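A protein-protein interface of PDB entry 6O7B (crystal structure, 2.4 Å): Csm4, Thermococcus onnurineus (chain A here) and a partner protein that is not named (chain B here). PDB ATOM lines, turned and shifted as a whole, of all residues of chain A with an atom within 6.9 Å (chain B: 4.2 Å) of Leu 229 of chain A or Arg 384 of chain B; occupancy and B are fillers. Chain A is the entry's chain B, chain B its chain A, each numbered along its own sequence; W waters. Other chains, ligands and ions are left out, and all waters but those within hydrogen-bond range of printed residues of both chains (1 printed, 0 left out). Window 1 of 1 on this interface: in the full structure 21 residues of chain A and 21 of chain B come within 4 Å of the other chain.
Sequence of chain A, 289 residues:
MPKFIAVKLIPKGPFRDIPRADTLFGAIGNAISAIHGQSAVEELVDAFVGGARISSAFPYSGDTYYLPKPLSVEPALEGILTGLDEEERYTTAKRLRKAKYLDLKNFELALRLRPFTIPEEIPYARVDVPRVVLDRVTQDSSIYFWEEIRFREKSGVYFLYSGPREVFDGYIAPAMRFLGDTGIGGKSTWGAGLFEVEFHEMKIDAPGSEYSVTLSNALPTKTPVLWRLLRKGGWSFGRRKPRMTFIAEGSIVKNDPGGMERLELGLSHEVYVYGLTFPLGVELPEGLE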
ATOM      1  N   TRP A 227      25.573  12.752 -17.722  1.00  0.00           N
ATOM      2  CA  TRP A 227      24.789  12.940 -18.963  1.00  0.00           C
ATOM      3  C   TRP A 227      24.116  11.638 -19.397  1.00  0.00           C
ATOM      4  O   TRP A 227      24.561  10.562 -18.953  1.00  0.00           O
ATOM      5  CB  TRP A 227      25.686  13.516 -20.060  1.00  0.00           C
ATOM      6  CG  TRP A 227      26.723  12.585 -20.614  1.00  0.00           C
ATOM      7  CD1 TRP A 227      26.558  11.719 -21.653  1.00  0.00           C
ATOM      8  CD2 TRP A 227      28.106  12.475 -20.219  1.00  0.00           C
ATOM      9  NE1 TRP A 227      27.726  11.064 -21.919  1.00  0.00           N
ATOM     10  CE2 TRP A 227      28.695  11.502 -21.055  1.00  0.00           C
ATOM     11  CE3 TRP A 227      28.905  13.084 -19.239  1.00  0.00           C
ATOM     12  CZ2 TRP A 227      30.038  11.137 -20.947  1.00  0.00           C
ATOM     13  CZ3 TRP A 227      30.232  12.720 -19.130  1.00  0.00           C
ATOM     14  CH2 TRP A 227      30.791  11.759 -19.977  1.00  0.00           C
ATOM     15  N   ARG A 228      23.036  11.782 -20.173  1.00  0.00           N
ATOM     16  CA  ARG A 228      22.472  10.762 -21.090  1.00  0.00           C
ATOM     17  C   ARG A 228      22.651  11.276 -22.520  1.00  0.00           C
ATOM     18  O   ARG A 228      22.399  12.477 -22.757  1.00  0.00           O
ATOM     19  CB  ARG A 228      20.983  10.519 -20.817  1.00  0.00           C
ATOM     20  CG  ARG A 228      20.666  10.021 -19.416  1.00  0.00           C
ATOM     21  CD  ARG A 228      19.311   9.337 -19.333  1.00  0.00           C
ATOM     22  NE  ARG A 228      18.273   9.971 -20.146  1.00  0.00           N
ATOM     23  CZ  ARG A 228      17.616  11.091 -19.836  1.00  0.00           C
ATOM     24  NH1 ARG A 228      16.692  11.558 -20.662  1.00  0.00           N
ATOM     25  NH2 ARG A 228      17.883  11.750 -18.721  1.00  0.00           N
ATOM     26  N   LEU A 229      23.069  10.407 -23.438  1.00  0.00           N
ATOM     27  CA  LEU A 229      23.203  10.755 -24.875  1.00  0.00           C
ATOM     28  C   LEU A 229      21.835  10.682 -25.546  1.00  0.00           C
ATOM     29  O   LEU A 229      20.925  10.022 -25.013  1.00  0.00           O
ATOM     30  CB  LEU A 229      24.184   9.808 -25.568  1.00  0.00           C
ATOM     31  CG  LEU A 229      25.625   9.879 -25.078  1.00  0.00           C
ATOM     32  CD1 LEU A 229      26.461   8.808 -25.752  1.00  0.00           C
ATOM     33  CD2 LEU A 229      26.222  11.261 -25.317  1.00  0.00           C
ATOM     34  N   LEU A 230      21.750  11.314 -26.711  1.00  0.00           N
ATOM     35  CA  LEU A 230      20.511  11.550 -27.485  1.00  0.00           C
ATOM     36  C   LEU A 230      20.927  11.692 -28.952  1.00  0.00           C
ATOM     37  O   LEU A 230      21.445  12.771 -29.317  1.00  0.00           O
ATOM     38  CB  LEU A 230      19.867  12.825 -26.931  1.00  0.00           C
ATOM     39  CG  LEU A 230      18.345  12.914 -26.995  1.00  0.00           C
ATOM     40  CD1 LEU A 230      17.698  11.913 -26.047  1.00  0.00           C
ATOM     41  CD2 LEU A 230      17.894  14.329 -26.665  1.00  0.00           C
ATOM     42  N   ARG A 231      20.772  10.620 -29.736  1.00  0.00           N
ATOM     43  CA  ARG A 231      21.211  10.532 -31.157  1.00  0.00           C
ATOM     44  C   ARG A 231      20.090  11.062 -32.064  1.00  0.00           C
ATOM     45  O   ARG A 231      18.940  10.618 -31.892  1.00  0.00           O
ATOM     46  CB  ARG A 231      21.582   9.081 -31.482  1.00  0.00           C
ATOM     47  CG  ARG A 231      22.251   8.875 -32.834  1.00  0.00           C
ATOM     48  CD  ARG A 231      23.767   8.965 -32.783  1.00  0.00           C
ATOM     49  NE  ARG A 231      24.344   9.147 -34.112  1.00  0.00           N
ATOM     50  CZ  ARG A 231      25.643   9.279 -34.374  1.00  0.00           C
ATOM     51  NH1 ARG A 231      26.536   9.245 -33.397  1.00  0.00           N
ATOM     52  NH2 ARG A 231      26.050   9.442 -35.623  1.00  0.00           N
ATOM     53  N   THR A 245      24.897  14.294 -32.061  1.00  0.00           N
ATOM     54  CA  THR A 245      24.970  13.715 -30.691  1.00  0.00           C
ATOM     55  C   THR A 245      24.778  14.831 -29.650  1.00  0.00           C
ATOM     56  O   THR A 245      25.707  15.641 -29.436  1.00  0.00           O
ATOM     57  CB  THR A 245      26.252  12.897 -30.496  1.00  0.00           C
ATOM     58  OG1 THR A 245      27.384  13.725 -30.765  1.00  0.00           O
ATOM     59  CG2 THR A 245      26.296  11.675 -31.387  1.00  0.00           C
ATOM     60  N   PHE A 246      23.595  14.854 -29.034  1.00  0.00           N
ATOM     61  CA  PHE A 246      23.181  15.795 -27.965  1.00  0.00           C
ATOM     62  C   PHE A 246      23.308  15.112 -26.600  1.00  0.00           C
ATOM     63  O   PHE A 246      23.179  13.872 -26.535  1.00  0.00           O
ATOM     64  CB  PHE A 246      21.718  16.207 -28.149  1.00  0.00           C
ATOM     65  CG  PHE A 246      21.417  17.148 -29.287  1.00  0.00           C
ATOM     66  CD1 PHE A 246      21.335  18.515 -29.069  1.00  0.00           C
ATOM     67  CD2 PHE A 246      21.149  16.671 -30.561  1.00  0.00           C
ATOM     68  CE1 PHE A 246      21.022  19.383 -30.102  1.00  0.00           C
ATOM     69  CE2 PHE A 246      20.837  17.542 -31.593  1.00  0.00           C
ATOM     70  CZ  PHE A 246      20.771  18.895 -31.361  1.00  0.00           C
ATOM     71  N   ILE A 247      23.517  15.900 -25.541  1.00  0.00           N
ATOM     72  CA  ILE A 247      23.239  15.476 -24.138  1.00  0.00           C
ATOM     73  C   ILE A 247      21.786  15.846 -23.804  1.00  0.00           C
ATOM     74  O   ILE A 247      21.278  16.853 -24.333  1.00  0.00           O
ATOM     75  CB  ILE A 247      24.254  16.057 -23.132  1.00  0.00           C
ATOM     76  CG1 ILE A 247      24.205  17.585 -23.036  1.00  0.00           C
ATOM     77  CG2 ILE A 247      25.651  15.543 -23.458  1.00  0.00           C
ATOM     78  CD1 ILE A 247      24.962  18.146 -21.859  1.00  0.00           C
ATOM     79  N   ALA A 248      21.142  15.030 -22.970  1.00  0.00           N
ATOM     80  CA  ALA A 248      19.702  15.114 -22.644  1.00  0.00           C
ATOM     81  C   ALA A 248      19.449  16.177 -21.571  1.00  0.00           C
ATOM     82  O   ALA A 248      20.366  16.477 -20.773  1.00  0.00           O
ATOM     83  CB  ALA A 248      19.200  13.771 -22.179  1.00  0.00           C
ATOM     84  N   SER A 251      21.028  16.550 -17.852  1.00  0.00           N
ATOM     85  CA  SER A 251      22.501  16.357 -17.853  1.00  0.00           C
ATOM     86  C   SER A 251      23.136  17.467 -17.013  1.00  0.00           C
ATOM     87  O   SER A 251      22.463  18.499 -16.789  1.00  0.00           O
ATOM     88  CB  SER A 251      23.061  16.327 -19.251  1.00  0.00           C
ATOM     89  OG  SER A 251      22.465  15.288 -20.014  1.00  0.00           O
ATOM     90  N   SER B 255      25.340  -1.887 -20.749  1.00  0.00           N
ATOM     91  CA  SER B 255      24.083  -1.094 -20.676  1.00  0.00           C
ATOM     92  C   SER B 255      23.596  -0.774 -22.089  1.00  0.00           C
ATOM     93  O   SER B 255      24.446  -0.508 -22.969  1.00  0.00           O
ATOM     94  CB  SER B 255      24.242   0.155 -19.856  1.00  0.00           C
ATOM     95  OG  SER B 255      25.317   0.939 -20.334  1.00  0.00           O
ATOM     96  N   GLY B 256      22.271  -0.818 -22.274  1.00  0.00           N
ATOM     97  CA  GLY B 256      21.581  -0.702 -23.569  1.00  0.00           C
ATOM     98  C   GLY B 256      21.333  -2.056 -24.210  1.00  0.00           C
ATOM     99  O   GLY B 256      21.112  -2.092 -25.443  1.00  0.00           O
ATOM    100  N   SER B 341      25.734   4.669 -30.220  1.00  0.00           N
ATOM    101  CA  SER B 341      25.516   4.898 -28.768  1.00  0.00           C
ATOM    102  C   SER B 341      24.714   3.752 -28.123  1.00  0.00           C
ATOM    103  O   SER B 341      24.423   3.860 -26.915  1.00  0.00           O
ATOM    104  CB  SER B 341      24.836   6.232 -28.547  1.00  0.00           C
ATOM    105  OG  SER B 341      24.591   6.457 -27.165  1.00  0.00           O
ATOM    106  N   ASP B 342      24.375   2.697 -28.876  1.00  0.00           N
ATOM    107  CA  ASP B 342      23.379   1.663 -28.469  1.00  0.00           C
ATOM    108  C   ASP B 342      23.906   0.820 -27.303  1.00  0.00           C
ATOM    109  O   ASP B 342      23.218   0.757 -26.268  1.00  0.00           O
ATOM    110  CB  ASP B 342      22.998   0.743 -29.634  1.00  0.00           C
ATOM    111  CG  ASP B 342      21.791   1.220 -30.423  1.00  0.00           C
ATOM    112  OD1 ASP B 342      20.857   1.763 -29.794  1.00  0.00           O
ATOM    113  OD2 ASP B 342      21.792   1.038 -31.660  1.00  0.00           O
ATOM    114  N   TYR B 344      26.834   0.197 -24.638  1.00  0.00           N
ATOM    115  CA  TYR B 344      27.986   0.666 -23.830  1.00  0.00           C
ATOM    116  C   TYR B 344      28.453  -0.481 -22.930  1.00  0.00           C
ATOM    117  O   TYR B 344      27.622  -1.348 -22.582  1.00  0.00           O
ATOM    118  CB  TYR B 344      27.593   1.885 -22.994  1.00  0.00           C
ATOM    119  CG  TYR B 344      28.717   2.457 -22.173  1.00  0.00           C
ATOM    120  CD1 TYR B 344      29.902   2.844 -22.778  1.00  0.00           C
ATOM    121  CD2 TYR B 344      28.608   2.606 -20.800  1.00  0.00           C
ATOM    122  CE1 TYR B 344      30.949   3.369 -22.041  1.00  0.00           C
ATOM    123  CE2 TYR B 344      29.649   3.128 -20.047  1.00  0.00           C
ATOM    124  CZ  TYR B 344      30.821   3.512 -20.673  1.00  0.00           C
ATOM    125  OH  TYR B 344      31.863   4.026 -19.962  1.00  0.00           O
ATOM    126  N   ARG B 380      29.774   5.716 -13.789  1.00  0.00           N
ATOM    127  CA  ARG B 380      30.354   5.422 -15.131  1.00  0.00           C
ATOM    128  C   ARG B 380      29.218   5.293 -16.162  1.00  0.00           C
ATOM    129  O   ARG B 380      29.414   5.724 -17.319  1.00  0.00           O
ATOM    130  CB  ARG B 380      31.248   4.179 -15.038  1.00  0.00           C
ATOM    131  CG  ARG B 380      31.613   3.526 -16.365  1.00  0.00           C
ATOM    132  CD  ARG B 380      32.542   4.356 -17.218  1.00  0.00           C
ATOM    133  NE  ARG B 380      33.697   4.835 -16.479  1.00  0.00           N
ATOM    134  CZ  ARG B 380      34.333   5.982 -16.713  1.00  0.00           C
ATOM    135  NH1 ARG B 380      33.919   6.803 -17.669  1.00  0.00           N
ATOM    136  NH2 ARG B 380      35.378   6.312 -15.971  1.00  0.00           N
ATOM    137  N   LYS B 381      28.064   4.752 -15.763  1.00  0.00           N
ATOM    138  CA  LYS B 381      26.889   4.569 -16.660  1.00  0.00           C
ATOM    139  C   LYS B 381      26.217   5.919 -16.958  1.00  0.00           C
ATOM    140  O   LYS B 381      25.427   5.974 -17.919  1.00  0.00           O
ATOM    141  CB  LYS B 381      25.888   3.581 -16.056  1.00  0.00           C
ATOM    142  CG  LYS B 381      26.151   2.124 -16.408  1.00  0.00           C
ATOM    143  CD  LYS B 381      25.202   1.157 -15.733  1.00  0.00           C
ATOM    144  CE  LYS B 381      25.906  -0.074 -15.213  1.00  0.00           C
ATOM    145  NZ  LYS B 381      25.014  -0.891 -14.360  1.00  0.00           N
ATOM    146  N   LEU B 382      26.508   6.955 -16.163  1.00  0.00           N
ATOM    147  CA  LEU B 382      26.053   8.355 -16.382  1.00  0.00           C
ATOM    148  C   LEU B 382      27.168   9.167 -17.060  1.00  0.00           C
ATOM    149  O   LEU B 382      27.016  10.395 -17.162  1.00  0.00           O
ATOM    150  CB  LEU B 382      25.655   8.970 -15.036  1.00  0.00           C
ATOM    151  CG  LEU B 382      24.502   8.277 -14.309  1.00  0.00           C
ATOM    152  CD1 LEU B 382      24.356   8.801 -12.886  1.00  0.00           C
ATOM    153  CD2 LEU B 382      23.197   8.435 -15.072  1.00  0.00           C
ATOM    154  N   LYS B 383      28.244   8.506 -17.497  1.00  0.00           N
ATOM    155  CA  LYS B 383      29.355   9.114 -18.277  1.00  0.00           C
ATOM    156  C   LYS B 383      29.588   8.228 -19.501  1.00  0.00           C
ATOM    157  O   LYS B 383      30.752   7.913 -19.804  1.00  0.00           O
ATOM    158  CB  LYS B 383      30.605   9.265 -17.402  1.00  0.00           C
ATOM    159  CG  LYS B 383      30.399  10.094 -16.139  1.00  0.00           C
ATOM    160  CD  LYS B 383      31.500   9.955 -15.104  1.00  0.00           C
ATOM    161  CE  LYS B 383      32.570  11.024 -15.196  1.00  0.00           C
ATOM    162  NZ  LYS B 383      32.107  12.310 -14.625  1.00  0.00           N
ATOM    163  N   ARG B 384      28.505   7.841 -20.176  1.00  0.00           N
ATOM    164  CA  ARG B 384      28.533   6.759 -21.192  1.00  0.00           C
ATOM    165  C   ARG B 384      29.301   7.289 -22.410  1.00  0.00           C
ATOM    166  O   ARG B 384      28.983   8.398 -22.883  1.00  0.00           O
ATOM    167  CB  ARG B 384      27.122   6.226 -21.478  1.00  0.00           C
ATOM    168  CG  ARG B 384      26.619   6.425 -22.900  1.00  0.00           C
ATOM    169  CD  ARG B 384      25.895   5.230 -23.508  1.00  0.00           C
ATOM    170  NE  ARG B 384      24.995   4.498 -22.622  1.00  0.00           N
ATOM    171  CZ  ARG B 384      24.202   3.501 -23.007  1.00  0.00           C
ATOM    172  NH1 ARG B 384      24.172   3.113 -24.272  1.00  0.00           N
ATOM    173  NH2 ARG B 384      23.430   2.897 -22.122  1.00  0.00           N
ATOM    174  N   PHE B 385      30.316   6.534 -22.841  1.00  0.00           N
ATOM    175  CA  PHE B 385      31.224   6.828 -23.983  1.00  0.00           C
ATOM    176  C   PHE B 385      32.141   8.019 -23.654  1.00  0.00           C
ATOM    177  O   PHE B 385      32.731   8.587 -24.587  1.00  0.00           O
ATOM    178  CB  PHE B 385      30.411   7.011 -25.266  1.00  0.00           C
ATOM    179  CG  PHE B 385      29.764   5.744 -25.765  1.00  0.00           C
ATOM    180  CD1 PHE B 385      30.536   4.699 -26.244  1.00  0.00           C
ATOM    181  CD2 PHE B 385      28.390   5.587 -25.751  1.00  0.00           C
ATOM    182  CE1 PHE B 385      29.948   3.531 -26.705  1.00  0.00           C
ATOM    183  CE2 PHE B 385      27.802   4.417 -26.208  1.00  0.00           C
ATOM    184  CZ  PHE B 385      28.581   3.393 -26.690  1.00  0.00           C
ATOM    185  N   GLY B 386      32.319   8.338 -22.368  1.00  0.00           N
ATOM    186  CA  GLY B 386      33.218   9.409 -21.893  1.00  0.00           C
ATOM    187  C   GLY B 386      34.688   9.102 -22.146  1.00  0.00           C
ATOM    188  O   GLY B 386      35.517  10.002 -21.923  1.00  0.00           O
ATOM    189  N   PHE B 392      32.266  14.635 -28.844  1.00  0.00           N
ATOM    190  CA  PHE B 392      31.555  15.943 -28.884  1.00  0.00           C
ATOM    191  C   PHE B 392      32.251  16.896 -29.868  1.00  0.00           C
ATOM    192  O   PHE B 392      32.702  17.985 -29.449  1.00  0.00           O
ATOM    193  CB  PHE B 392      31.456  16.517 -27.467  1.00  0.00           C
ATOM    194  CG  PHE B 392      30.717  15.641 -26.485  1.00  0.00           C
ATOM    195  CD1 PHE B 392      29.406  15.251 -26.726  1.00  0.00           C
ATOM    196  CD2 PHE B 392      31.321  15.217 -25.310  1.00  0.00           C
ATOM    197  CE1 PHE B 392      28.720  14.458 -25.818  1.00  0.00           C
ATOM    198  CE2 PHE B 392      30.636  14.417 -24.408  1.00  0.00           C
ATOM    199  CZ  PHE B 392      29.338  14.040 -24.661  1.00  0.00           C
HETATM  200  O   HOH W   1      23.700   7.711 -22.354  1.00  0.00           O
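N of Trp 227 of chain A sits at hydrogen-bond distance from O of Leu 382 of chain B, at 2.8 Å.
NE1 of Trp 227 of chain A is in hydrogen-bond range of O of Arg 384 of chain B (3.1 Å).
The guanidinium group (NH2) of Arg 384 of chain B lies within hydrogen-bond range of the side-chain hydroxyl (OG) of Ser 255 of chain B (3.3 Å).
The backbone carbonyl oxygen of Ser 341 of chain B is in hydrogen-bond range of the guanidinium group of Arg 384 of chain B, at 2.8 Å.
O of Asp 342 of chain B sits at hydrogen-bond distance from NH1 of Arg 384 of chain B (3.2 Å).
Among the printed residues, pairs that only touch across the chains: Trp 227 of chain A with Lys 383 of chain B (3.3 Å), Leu 229 of chain A with Ser 341 of chain B (3.3 Å), Leu 229 of chain A with Arg 384 of chain B (3.7 Å), Trp 227 of chain A with Gly 386 of chain B (3.7 Å) and Leu 229 of chain A with Phe 385 of chain B (3.8 Å).
Of chain B, only Ser 341, Arg 384 and Phe 385 come within 4 Å of Leu 229 of chain A.
Arg 384 of chain B touches just these residues of chain A: Trp 227 and Leu 229.
Printed residues of chain A within 4 Å of Phe 385 of chain B: Leu 229 (3.8 Å).
Of the printed residues of chain A, Lys 383 of chain B touches Trp 227 (3.3 Å).
Of the printed residues of chain A, Ser 341 of chain B touches Leu 229.
The nearest residue of chain B that does not touch Leu 229 of chain A is Phe 392 of chain B (4.1 Å).
The nearest residue of chain A that does not touch Arg 384 of chain B is Arg 228 of chain A (6.3 Å).
Along chain B the printed residues that touch a printed residue of chain A span positions 341 to 386.
Hydrophobic or aromatic side chains of chain A that line the printed part of chain B: Trp 227 and Leu 229.
Among the printed residues, no Asp or Glu carboxylate lies within 4 Å of a Lys or Arg side-chain nitrogen of the other chain.
Water W1 bridges the backbone NH (N) of Leu 229 of chain A (3.0 Å) and the guanidinium group (NE) of Arg 384 of chain B (3.5 Å).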
